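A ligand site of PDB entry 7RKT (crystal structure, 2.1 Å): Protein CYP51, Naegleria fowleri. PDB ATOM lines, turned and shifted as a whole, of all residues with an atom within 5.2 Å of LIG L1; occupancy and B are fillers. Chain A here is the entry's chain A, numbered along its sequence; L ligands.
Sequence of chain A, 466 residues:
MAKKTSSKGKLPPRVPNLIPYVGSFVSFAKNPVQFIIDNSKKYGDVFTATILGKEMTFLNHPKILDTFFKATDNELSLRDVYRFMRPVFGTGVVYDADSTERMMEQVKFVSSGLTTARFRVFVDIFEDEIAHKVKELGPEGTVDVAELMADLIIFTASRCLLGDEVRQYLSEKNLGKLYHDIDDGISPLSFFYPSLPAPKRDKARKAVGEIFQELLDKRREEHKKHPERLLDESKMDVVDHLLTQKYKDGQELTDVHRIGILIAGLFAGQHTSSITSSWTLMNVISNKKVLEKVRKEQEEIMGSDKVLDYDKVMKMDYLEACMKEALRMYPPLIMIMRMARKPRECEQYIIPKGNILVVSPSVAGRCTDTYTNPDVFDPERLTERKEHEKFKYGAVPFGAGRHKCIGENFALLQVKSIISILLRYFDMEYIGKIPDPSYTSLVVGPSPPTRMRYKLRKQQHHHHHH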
ATOM      1  N   TYR A  82     -22.495  29.969 -12.764  1.00  0.00           N
ATOM      2  CA  TYR A  82     -22.625  29.203 -11.526  1.00  0.00           C
ATOM      3  C   TYR A  82     -24.081  28.846 -11.209  1.00  0.00           C
ATOM      4  O   TYR A  82     -24.389  28.362 -10.113  1.00  0.00           O
ATOM      5  CB  TYR A  82     -22.053  30.022 -10.372  1.00  0.00           C
ATOM      6  CG  TYR A  82     -20.589  30.353 -10.464  1.00  0.00           C
ATOM      7  CD1 TYR A  82     -19.659  29.352 -10.696  1.00  0.00           C
ATOM      8  CD2 TYR A  82     -20.126  31.633 -10.233  1.00  0.00           C
ATOM      9  CE1 TYR A  82     -18.299  29.632 -10.737  1.00  0.00           C
ATOM     10  CE2 TYR A  82     -18.780  31.937 -10.282  1.00  0.00           C
ATOM     11  CZ  TYR A  82     -17.869  30.923 -10.544  1.00  0.00           C
ATOM     12  OH  TYR A  82     -16.514  31.165 -10.593  1.00  0.00           O
ATOM     13  N   PHE A  84     -25.620  26.414 -12.413  1.00  0.00           N
ATOM     14  CA  PHE A  84     -25.616  24.955 -12.239  1.00  0.00           C
ATOM     15  C   PHE A  84     -25.641  24.494 -10.788  1.00  0.00           C
ATOM     16  O   PHE A  84     -26.023  23.364 -10.531  1.00  0.00           O
ATOM     17  CB  PHE A  84     -24.449  24.282 -13.005  1.00  0.00           C
ATOM     18  CG  PHE A  84     -23.106  24.420 -12.321  1.00  0.00           C
ATOM     19  CD1 PHE A  84     -22.287  25.487 -12.589  1.00  0.00           C
ATOM     20  CD2 PHE A  84     -22.652  23.434 -11.460  1.00  0.00           C
ATOM     21  CE1 PHE A  84     -21.072  25.617 -11.958  1.00  0.00           C
ATOM     22  CE2 PHE A  84     -21.438  23.542 -10.819  1.00  0.00           C
ATOM     23  CZ  PHE A  84     -20.626  24.621 -11.092  1.00  0.00           C
ATOM     24  N   MET A  85     -25.267  25.352  -9.832  1.00  0.00           N
ATOM     25  CA  MET A  85     -25.472  25.065  -8.392  1.00  0.00           C
ATOM     26  C   MET A  85     -26.911  25.054  -7.917  1.00  0.00           C
ATOM     27  O   MET A  85     -27.159  24.772  -6.734  1.00  0.00           O
ATOM     28  CB  MET A  85     -24.717  26.062  -7.508  1.00  0.00           C
ATOM     29  CG  MET A  85     -23.201  26.055  -7.675  1.00  0.00           C
ATOM     30  SD  MET A  85     -22.446  24.466  -7.389  1.00  0.00           S
ATOM     31  CE  MET A  85     -22.859  24.215  -5.662  1.00  0.00           C
ATOM     32  N   PHE A  89     -28.254  24.801  -3.961  1.00  0.00           N
ATOM     33  CA  PHE A  89     -28.771  25.990  -3.236  1.00  0.00           C
ATOM     34  C   PHE A  89     -30.303  26.140  -3.313  1.00  0.00           C
ATOM     35  O   PHE A  89     -30.886  26.719  -2.426  1.00  0.00           O
ATOM     36  CB  PHE A  89     -28.108  27.301  -3.721  1.00  0.00           C
ATOM     37  CG  PHE A  89     -26.595  27.331  -3.612  1.00  0.00           C
ATOM     38  CD1 PHE A  89     -25.902  26.605  -2.639  1.00  0.00           C
ATOM     39  CD2 PHE A  89     -25.866  28.072  -4.513  1.00  0.00           C
ATOM     40  CE1 PHE A  89     -24.512  26.655  -2.565  1.00  0.00           C
ATOM     41  CE2 PHE A  89     -24.457  28.111  -4.449  1.00  0.00           C
ATOM     42  CZ  PHE A  89     -23.796  27.407  -3.462  1.00  0.00           C
ATOM     43  N   VAL A  94     -29.521  32.898  -4.870  1.00  0.00           N
ATOM     44  CA  VAL A  94     -28.130  33.101  -5.155  1.00  0.00           C
ATOM     45  C   VAL A  94     -28.034  33.211  -6.680  1.00  0.00           C
ATOM     46  O   VAL A  94     -28.607  34.147  -7.228  1.00  0.00           O
ATOM     47  CB  VAL A  94     -27.246  31.990  -4.499  1.00  0.00           C
ATOM     48  CG1 VAL A  94     -25.789  32.338  -4.673  1.00  0.00           C
ATOM     49  CG2 VAL A  94     -27.529  31.836  -3.017  1.00  0.00           C
ATOM     50  N   TYR A  95     -27.404  32.254  -7.389  1.00  0.00           N
ATOM     51  CA  TYR A  95     -27.095  32.486  -8.814  1.00  0.00           C
ATOM     52  C   TYR A  95     -28.267  32.177  -9.703  1.00  0.00           C
ATOM     53  O   TYR A  95     -28.211  32.434 -10.917  1.00  0.00           O
ATOM     54  CB  TYR A  95     -25.899  31.670  -9.286  1.00  0.00           C
ATOM     55  CG  TYR A  95     -24.716  31.893  -8.437  1.00  0.00           C
ATOM     56  CD1 TYR A  95     -24.115  33.161  -8.367  1.00  0.00           C
ATOM     57  CD2 TYR A  95     -24.190  30.854  -7.653  1.00  0.00           C
ATOM     58  CE1 TYR A  95     -23.010  33.382  -7.570  1.00  0.00           C
ATOM     59  CE2 TYR A  95     -23.074  31.057  -6.874  1.00  0.00           C
ATOM     60  CZ  TYR A  95     -22.504  32.320  -6.817  1.00  0.00           C
ATOM     61  OH  TYR A  95     -21.402  32.489  -6.015  1.00  0.00           O
ATOM     62  N   VAL A 107     -27.480  37.741   0.025  1.00  0.00           N
ATOM     63  CA  VAL A 107     -26.157  37.737   0.559  1.00  0.00           C
ATOM     64  C   VAL A 107     -26.100  38.575   1.824  1.00  0.00           C
ATOM     65  O   VAL A 107     -25.598  38.087   2.836  1.00  0.00           O
ATOM     66  CB  VAL A 107     -25.154  38.262  -0.478  1.00  0.00           C
ATOM     67  CG1 VAL A 107     -23.809  38.584   0.151  1.00  0.00           C
ATOM     68  CG2 VAL A 107     -25.029  37.203  -1.553  1.00  0.00           C
ATOM     69  N   VAL A 110     -27.098  36.900   5.080  1.00  0.00           N
ATOM     70  CA  VAL A 110     -26.096  36.061   5.695  1.00  0.00           C
ATOM     71  C   VAL A 110     -25.113  36.970   6.445  1.00  0.00           C
ATOM     72  O   VAL A 110     -24.832  36.764   7.645  1.00  0.00           O
ATOM     73  CB  VAL A 110     -25.376  35.159   4.662  1.00  0.00           C
ATOM     74  CG1 VAL A 110     -24.225  34.394   5.293  1.00  0.00           C
ATOM     75  CG2 VAL A 110     -26.377  34.182   4.060  1.00  0.00           C
ATOM     76  N   ILE A 261     -30.908  29.773   1.232  1.00  0.00           N
ATOM     77  CA  ILE A 261     -29.906  30.695   1.700  1.00  0.00           C
ATOM     78  C   ILE A 261     -29.055  30.082   2.855  1.00  0.00           C
ATOM     79  O   ILE A 261     -27.836  30.153   2.856  1.00  0.00           O
ATOM     80  CB  ILE A 261     -30.560  32.056   2.097  1.00  0.00           C
ATOM     81  CG1 ILE A 261     -31.038  32.801   0.861  1.00  0.00           C
ATOM     82  CG2 ILE A 261     -29.559  32.945   2.833  1.00  0.00           C
ATOM     83  CD1 ILE A 261     -32.103  33.849   1.131  1.00  0.00           C
ATOM     84  N   ALA A 264     -26.886  27.319   1.477  1.00  0.00           N
ATOM     85  CA  ALA A 264     -25.754  27.976   0.796  1.00  0.00           C
ATOM     86  C   ALA A 264     -24.749  28.535   1.797  1.00  0.00           C
ATOM     87  O   ALA A 264     -23.530  28.432   1.595  1.00  0.00           O
ATOM     88  CB  ALA A 264     -26.227  29.070  -0.135  1.00  0.00           C
ATOM     89  N   GLY A 265     -25.275  29.086   2.898  1.00  0.00           N
ATOM     90  CA  GLY A 265     -24.439  29.707   3.935  1.00  0.00           C
ATOM     91  C   GLY A 265     -23.471  28.749   4.601  1.00  0.00           C
ATOM     92  O   GLY A 265     -22.328  29.059   4.775  1.00  0.00           O
ATOM     93  N   PHE A 267     -22.826  25.547   3.370  1.00  0.00           N
ATOM     94  CA  PHE A 267     -22.031  25.074   2.253  1.00  0.00           C
ATOM     95  C   PHE A 267     -20.797  25.997   2.038  1.00  0.00           C
ATOM     96  O   PHE A 267     -19.699  25.515   1.993  1.00  0.00           O
ATOM     97  CB  PHE A 267     -22.894  25.043   1.000  1.00  0.00           C
ATOM     98  CG  PHE A 267     -22.235  24.380  -0.173  1.00  0.00           C
ATOM     99  CD1 PHE A 267     -21.484  25.130  -1.081  1.00  0.00           C
ATOM    100  CD2 PHE A 267     -22.389  23.015  -0.392  1.00  0.00           C
ATOM    101  CE1 PHE A 267     -20.886  24.500  -2.183  1.00  0.00           C
ATOM    102  CE2 PHE A 267     -21.811  22.385  -1.486  1.00  0.00           C
ATOM    103  CZ  PHE A 267     -21.054  23.124  -2.390  1.00  0.00           C
ATOM    104  N   ALA A 268     -20.997  27.306   1.946  1.00  0.00           N
ATOM    105  CA  ALA A 268     -19.889  28.240   1.681  1.00  0.00           C
ATOM    106  C   ALA A 268     -18.693  27.942   2.572  1.00  0.00           C
ATOM    107  O   ALA A 268     -17.590  27.588   2.089  1.00  0.00           O
ATOM    108  CB  ALA A 268     -20.323  29.689   1.880  1.00  0.00           C
ATOM    109  N   GLY A 269     -18.964  28.018   3.868  1.00  0.00           N
ATOM    110  CA  GLY A 269     -17.953  27.872   4.910  1.00  0.00           C
ATOM    111  C   GLY A 269     -18.156  26.595   5.664  1.00  0.00           C
ATOM    112  O   GLY A 269     -18.355  26.585   6.892  1.00  0.00           O
ATOM    113  N   THR A 272     -14.323  25.146   2.401  1.00  0.00           N
ATOM    114  CA  THR A 272     -13.196  26.078   2.242  1.00  0.00           C
ATOM    115  C   THR A 272     -12.469  26.365   3.568  1.00  0.00           C
ATOM    116  O   THR A 272     -11.258  26.263   3.620  1.00  0.00           O
ATOM    117  CB  THR A 272     -13.636  27.430   1.695  1.00  0.00           C
ATOM    118  OG1 THR A 272     -14.758  27.886   2.448  1.00  0.00           O
ATOM    119  CG2 THR A 272     -14.001  27.318   0.285  1.00  0.00           C
ATOM    120  N   LEU A 333     -10.677  27.345  -3.594  1.00  0.00           N
ATOM    121  CA  LEU A 333     -11.317  27.701  -4.852  1.00  0.00           C
ATOM    122  C   LEU A 333     -10.161  28.052  -5.810  1.00  0.00           C
ATOM    123  O   LEU A 333      -9.634  29.151  -5.833  1.00  0.00           O
ATOM    124  CB  LEU A 333     -12.308  28.846  -4.693  1.00  0.00           C
ATOM    125  CG  LEU A 333     -13.306  28.665  -3.534  1.00  0.00           C
ATOM    126  CD1 LEU A 333     -14.244  29.853  -3.312  1.00  0.00           C
ATOM    127  CD2 LEU A 333     -14.090  27.372  -3.693  1.00  0.00           C
ATOM    128  N   CYS A 405     -15.348  38.097  -0.876  1.00  0.00           N
ATOM    129  CA  CYS A 405     -15.920  37.185   0.083  1.00  0.00           C
ATOM    130  C   CYS A 405     -16.546  37.929   1.241  1.00  0.00           C
ATOM    131  O   CYS A 405     -15.883  38.655   1.939  1.00  0.00           O
ATOM    132  CB  CYS A 405     -14.845  36.234   0.602  1.00  0.00           C
ATOM    133  SG  CYS A 405     -15.542  34.876   1.654  1.00  0.00           S
ATOM    134  N   LEU A 442     -15.106  19.824  -6.436  1.00  0.00           N
ATOM    135  CA  LEU A 442     -15.413  21.244  -6.669  1.00  0.00           C
ATOM    136  C   LEU A 442     -14.466  22.157  -5.871  1.00  0.00           C
ATOM    137  O   LEU A 442     -13.950  23.148  -6.424  1.00  0.00           O
ATOM    138  CB  LEU A 442     -16.867  21.518  -6.278  1.00  0.00           C
ATOM    139  CG  LEU A 442     -17.667  22.536  -7.070  1.00  0.00           C
ATOM    140  CD1 LEU A 442     -17.490  22.399  -8.581  1.00  0.00           C
ATOM    141  CD2 LEU A 442     -19.133  22.377  -6.660  1.00  0.00           C
ATOM    142  N   VAL A 443     -14.275  21.791  -4.595  1.00  0.00           N
ATOM    143  CA  VAL A 443     -13.412  22.495  -3.630  1.00  0.00           C
ATOM    144  C   VAL A 443     -12.192  21.638  -3.344  1.00  0.00           C
ATOM    145  O   VAL A 443     -12.296  20.566  -2.746  1.00  0.00           O
ATOM    146  CB  VAL A 443     -14.158  22.769  -2.312  1.00  0.00           C
ATOM    147  CG1 VAL A 443     -13.355  23.707  -1.409  1.00  0.00           C
ATOM    148  CG2 VAL A 443     -15.540  23.374  -2.592  1.00  0.00           C
HETATM  149  C1  LIG L   1     -19.507  28.389  -4.607  1.00  0.00           C
HETATM  150  C2  LIG L   1     -20.942  29.719  -1.966  1.00  0.00           C
HETATM  151  C3  LIG L   1     -21.788  30.929  -1.901  1.00  0.00           C
HETATM  152  C4  LIG L   1     -21.766  31.851  -2.937  1.00  0.00           C
HETATM  153  C5  LIG L   1     -22.631  32.943  -2.888  1.00  0.00           C
HETATM  154  C6  LIG L   1     -22.651  31.142  -0.832  1.00  0.00           C
HETATM  155  C7  LIG L   1     -24.478  32.462   0.415  1.00  0.00           C
HETATM  156  C8  LIG L   1     -17.074  29.344  -0.865  1.00  0.00           C
HETATM  157  C9  LIG L   1     -16.712  30.330   0.017  1.00  0.00           C
HETATM  158 CL1  LIG L   1     -20.190  26.753  -8.750  1.00  0.00          CL
HETATM  159  C10 LIG L   1     -19.928  27.373  -7.159  1.00  0.00           C
HETATM  160  C11 LIG L   1     -20.313  28.674  -6.858  1.00  0.00           C
HETATM  161  C12 LIG L   1     -20.089  29.176  -5.584  1.00  0.00           C
HETATM  162  C13 LIG L   1     -19.128  27.090  -4.965  1.00  0.00           C
HETATM  163  C14 LIG L   1     -19.340  26.555  -6.232  1.00  0.00           C
HETATM  164 CL2  LIG L   1     -18.363  26.035  -3.814  1.00  0.00          CL
HETATM  165  C15 LIG L   1     -19.210  28.878  -3.249  1.00  0.00           C
HETATM  166  O1  LIG L   1     -20.091  29.783  -3.027  1.00  0.00           O
HETATM  167  O2  LIG L   1     -21.142  28.762  -1.225  1.00  0.00           O
HETATM  168  C16 LIG L   1     -23.504  33.116  -1.818  1.00  0.00           C
HETATM  169  C17 LIG L   1     -23.521  32.230  -0.761  1.00  0.00           C
HETATM  170  F1  LIG L   1     -24.299  31.663   1.501  1.00  0.00           F
HETATM  171  F2  LIG L   1     -24.387  33.714   0.922  1.00  0.00           F
HETATM  172  F3  LIG L   1     -25.802  32.353   0.141  1.00  0.00           F
HETATM  173  C18 LIG L   1     -17.804  29.369  -3.345  1.00  0.00           C
HETATM  174  N1  LIG L   1     -17.342  29.978  -2.057  1.00  0.00           N
HETATM  175  N2  LIG L   1     -16.753  31.585  -0.602  1.00  0.00           N
HETATM  176  C19 LIG L   1     -17.147  31.294  -1.822  1.00  0.00           C
HETATM  177  C1  LG2 L   2     -16.922  34.927  -2.376  1.00  0.00           C
HETATM  178  C2  LG2 L   2     -13.090  32.434  -0.808  1.00  0.00           C
HETATM  179  C3  LG2 L   2     -15.393  31.559   3.363  1.00  0.00           C
HETATM  180  C4  LG2 L   2     -19.320  33.547   1.553  1.00  0.00           C
HETATM  181  C5  LG2 L   2     -15.684  34.360  -2.264  1.00  0.00           C
HETATM  182  C6  LG2 L   2     -14.681  34.457  -3.260  1.00  0.00           C
HETATM  183  C7  LG2 L   2     -13.610  33.748  -2.820  1.00  0.00           C
HETATM  184  C8  LG2 L   2     -13.956  33.205  -1.566  1.00  0.00           C
HETATM  185  C9  LG2 L   2     -12.302  33.548  -3.559  1.00  0.00           C
HETATM  186  C10 LG2 L   2     -14.797  35.179  -4.563  1.00  0.00           C
HETATM  187  C11 LG2 L   2     -15.678  34.357  -5.544  1.00  0.00           C
HETATM  188  C12 LG2 L   2     -15.818  35.008  -6.940  1.00  0.00           C
HETATM  189  O1  LG2 L   2     -16.447  34.419  -7.881  1.00  0.00           O
HETATM  190  O2  LG2 L   2     -15.306  36.132  -7.182  1.00  0.00           O
HETATM  191  C13 LG2 L   2     -13.392  31.974   0.467  1.00  0.00           C
HETATM  192  C14 LG2 L   2     -12.444  31.289   1.264  1.00  0.00           C
HETATM  193  C15 LG2 L   2     -13.077  30.994   2.452  1.00  0.00           C
HETATM  194  C16 LG2 L   2     -14.433  31.592   2.350  1.00  0.00           C
HETATM  195  C17 LG2 L   2     -11.048  30.897   0.876  1.00  0.00           C
HETATM  196  C18 LG2 L   2     -12.555  30.370   3.673  1.00  0.00           C
HETATM  197  C19 LG2 L   2     -11.266  30.339   3.994  1.00  0.00           C
HETATM  198  C20 LG2 L   2     -16.683  32.032   3.236  1.00  0.00           C
HETATM  199  C21 LG2 L   2     -17.699  31.834   4.183  1.00  0.00           C
HETATM  200  C22 LG2 L   2     -18.853  32.424   3.661  1.00  0.00           C
HETATM  201  C23 LG2 L   2     -18.469  32.937   2.383  1.00  0.00           C
HETATM  202  C24 LG2 L   2     -17.460  31.175   5.517  1.00  0.00           C
HETATM  203  C25 LG2 L   2     -20.198  32.594   4.209  1.00  0.00           C
HETATM  204  C26 LG2 L   2     -20.560  32.298   5.465  1.00  0.00           C
HETATM  205  C27 LG2 L   2     -18.933  34.074   0.357  1.00  0.00           C
HETATM  206  C28 LG2 L   2     -19.909  34.806  -0.406  1.00  0.00           C
HETATM  207  C29 LG2 L   2     -19.254  35.221  -1.484  1.00  0.00           C
HETATM  208  C30 LG2 L   2     -17.893  34.707  -1.394  1.00  0.00           C
HETATM  209  C31 LG2 L   2     -21.368  35.079  -0.109  1.00  0.00           C
HETATM  210  C32 LG2 L   2     -19.935  35.966  -2.613  1.00  0.00           C
HETATM  211  C33 LG2 L   2     -19.540  37.423  -2.666  1.00  0.00           C
HETATM  212  C34 LG2 L   2     -20.517  38.131  -3.615  1.00  0.00           C
HETATM  213  O3  LG2 L   2     -21.061  39.220  -3.249  1.00  0.00           O
HETATM  214  O4  LG2 L   2     -20.763  37.614  -4.751  1.00  0.00           O
HETATM  215  N1  LG2 L   2     -15.189  33.595  -1.251  1.00  0.00           N
HETATM  216  N2  LG2 L   2     -14.546  32.143   1.134  1.00  0.00           N
HETATM  217  N3  LG2 L   2     -17.219  32.640   2.158  1.00  0.00           N
HETATM  218  N4  LG2 L   2     -17.718  34.027  -0.232  1.00  0.00           N
HETATM  219 FE1  LG2 L   2     -16.193  33.146   0.433  1.00  0.00          FE
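SG of Cys 405 is bound to FE1 of LG2 L2, 2.2 Å away.
O2 of LIG L1 lies close to N of Ala 268, at 3.5 Å.
A nitrogen (N2) of LIG L1 binds an iron atom (FE1) of LG2 L2 (2.0 Å).
O of Ala 268 is in hydrogen-bond range of OG1 of Thr 272, 2.9 Å away.
A fluorine (F1) of LIG L1 sits close to the backbone carbonyl oxygen of Ala 264, 3.3 Å away.
The backbone NH (N) of Gly 265 sits close to a fluorine (F1) of LIG L1 (3.1 Å).
Residues that only touch LIG L1: Tyr 95 (3.2 Å), Phe 84 (3.2 Å), Met 85 (3.3 Å), Tyr 82 (3.3 Å), Leu 333 (3.3 Å), Phe 267 (3.4 Å), Val 94 (3.6 Å), Phe 89 (3.7 Å), Val 110 (3.7 Å) and Thr 272 (3.9 Å).
Hydrophobic or aromatic side chains that line LIG L1: Tyr 82, Phe 84, Met 85, Phe 89, Val 94, Tyr 95, Val 110, Ala 264, Phe 267, Ala 268 and Leu 333.
The nearest printed residue that does not touch LIG L1 is Ile 261 (4.04 Å).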
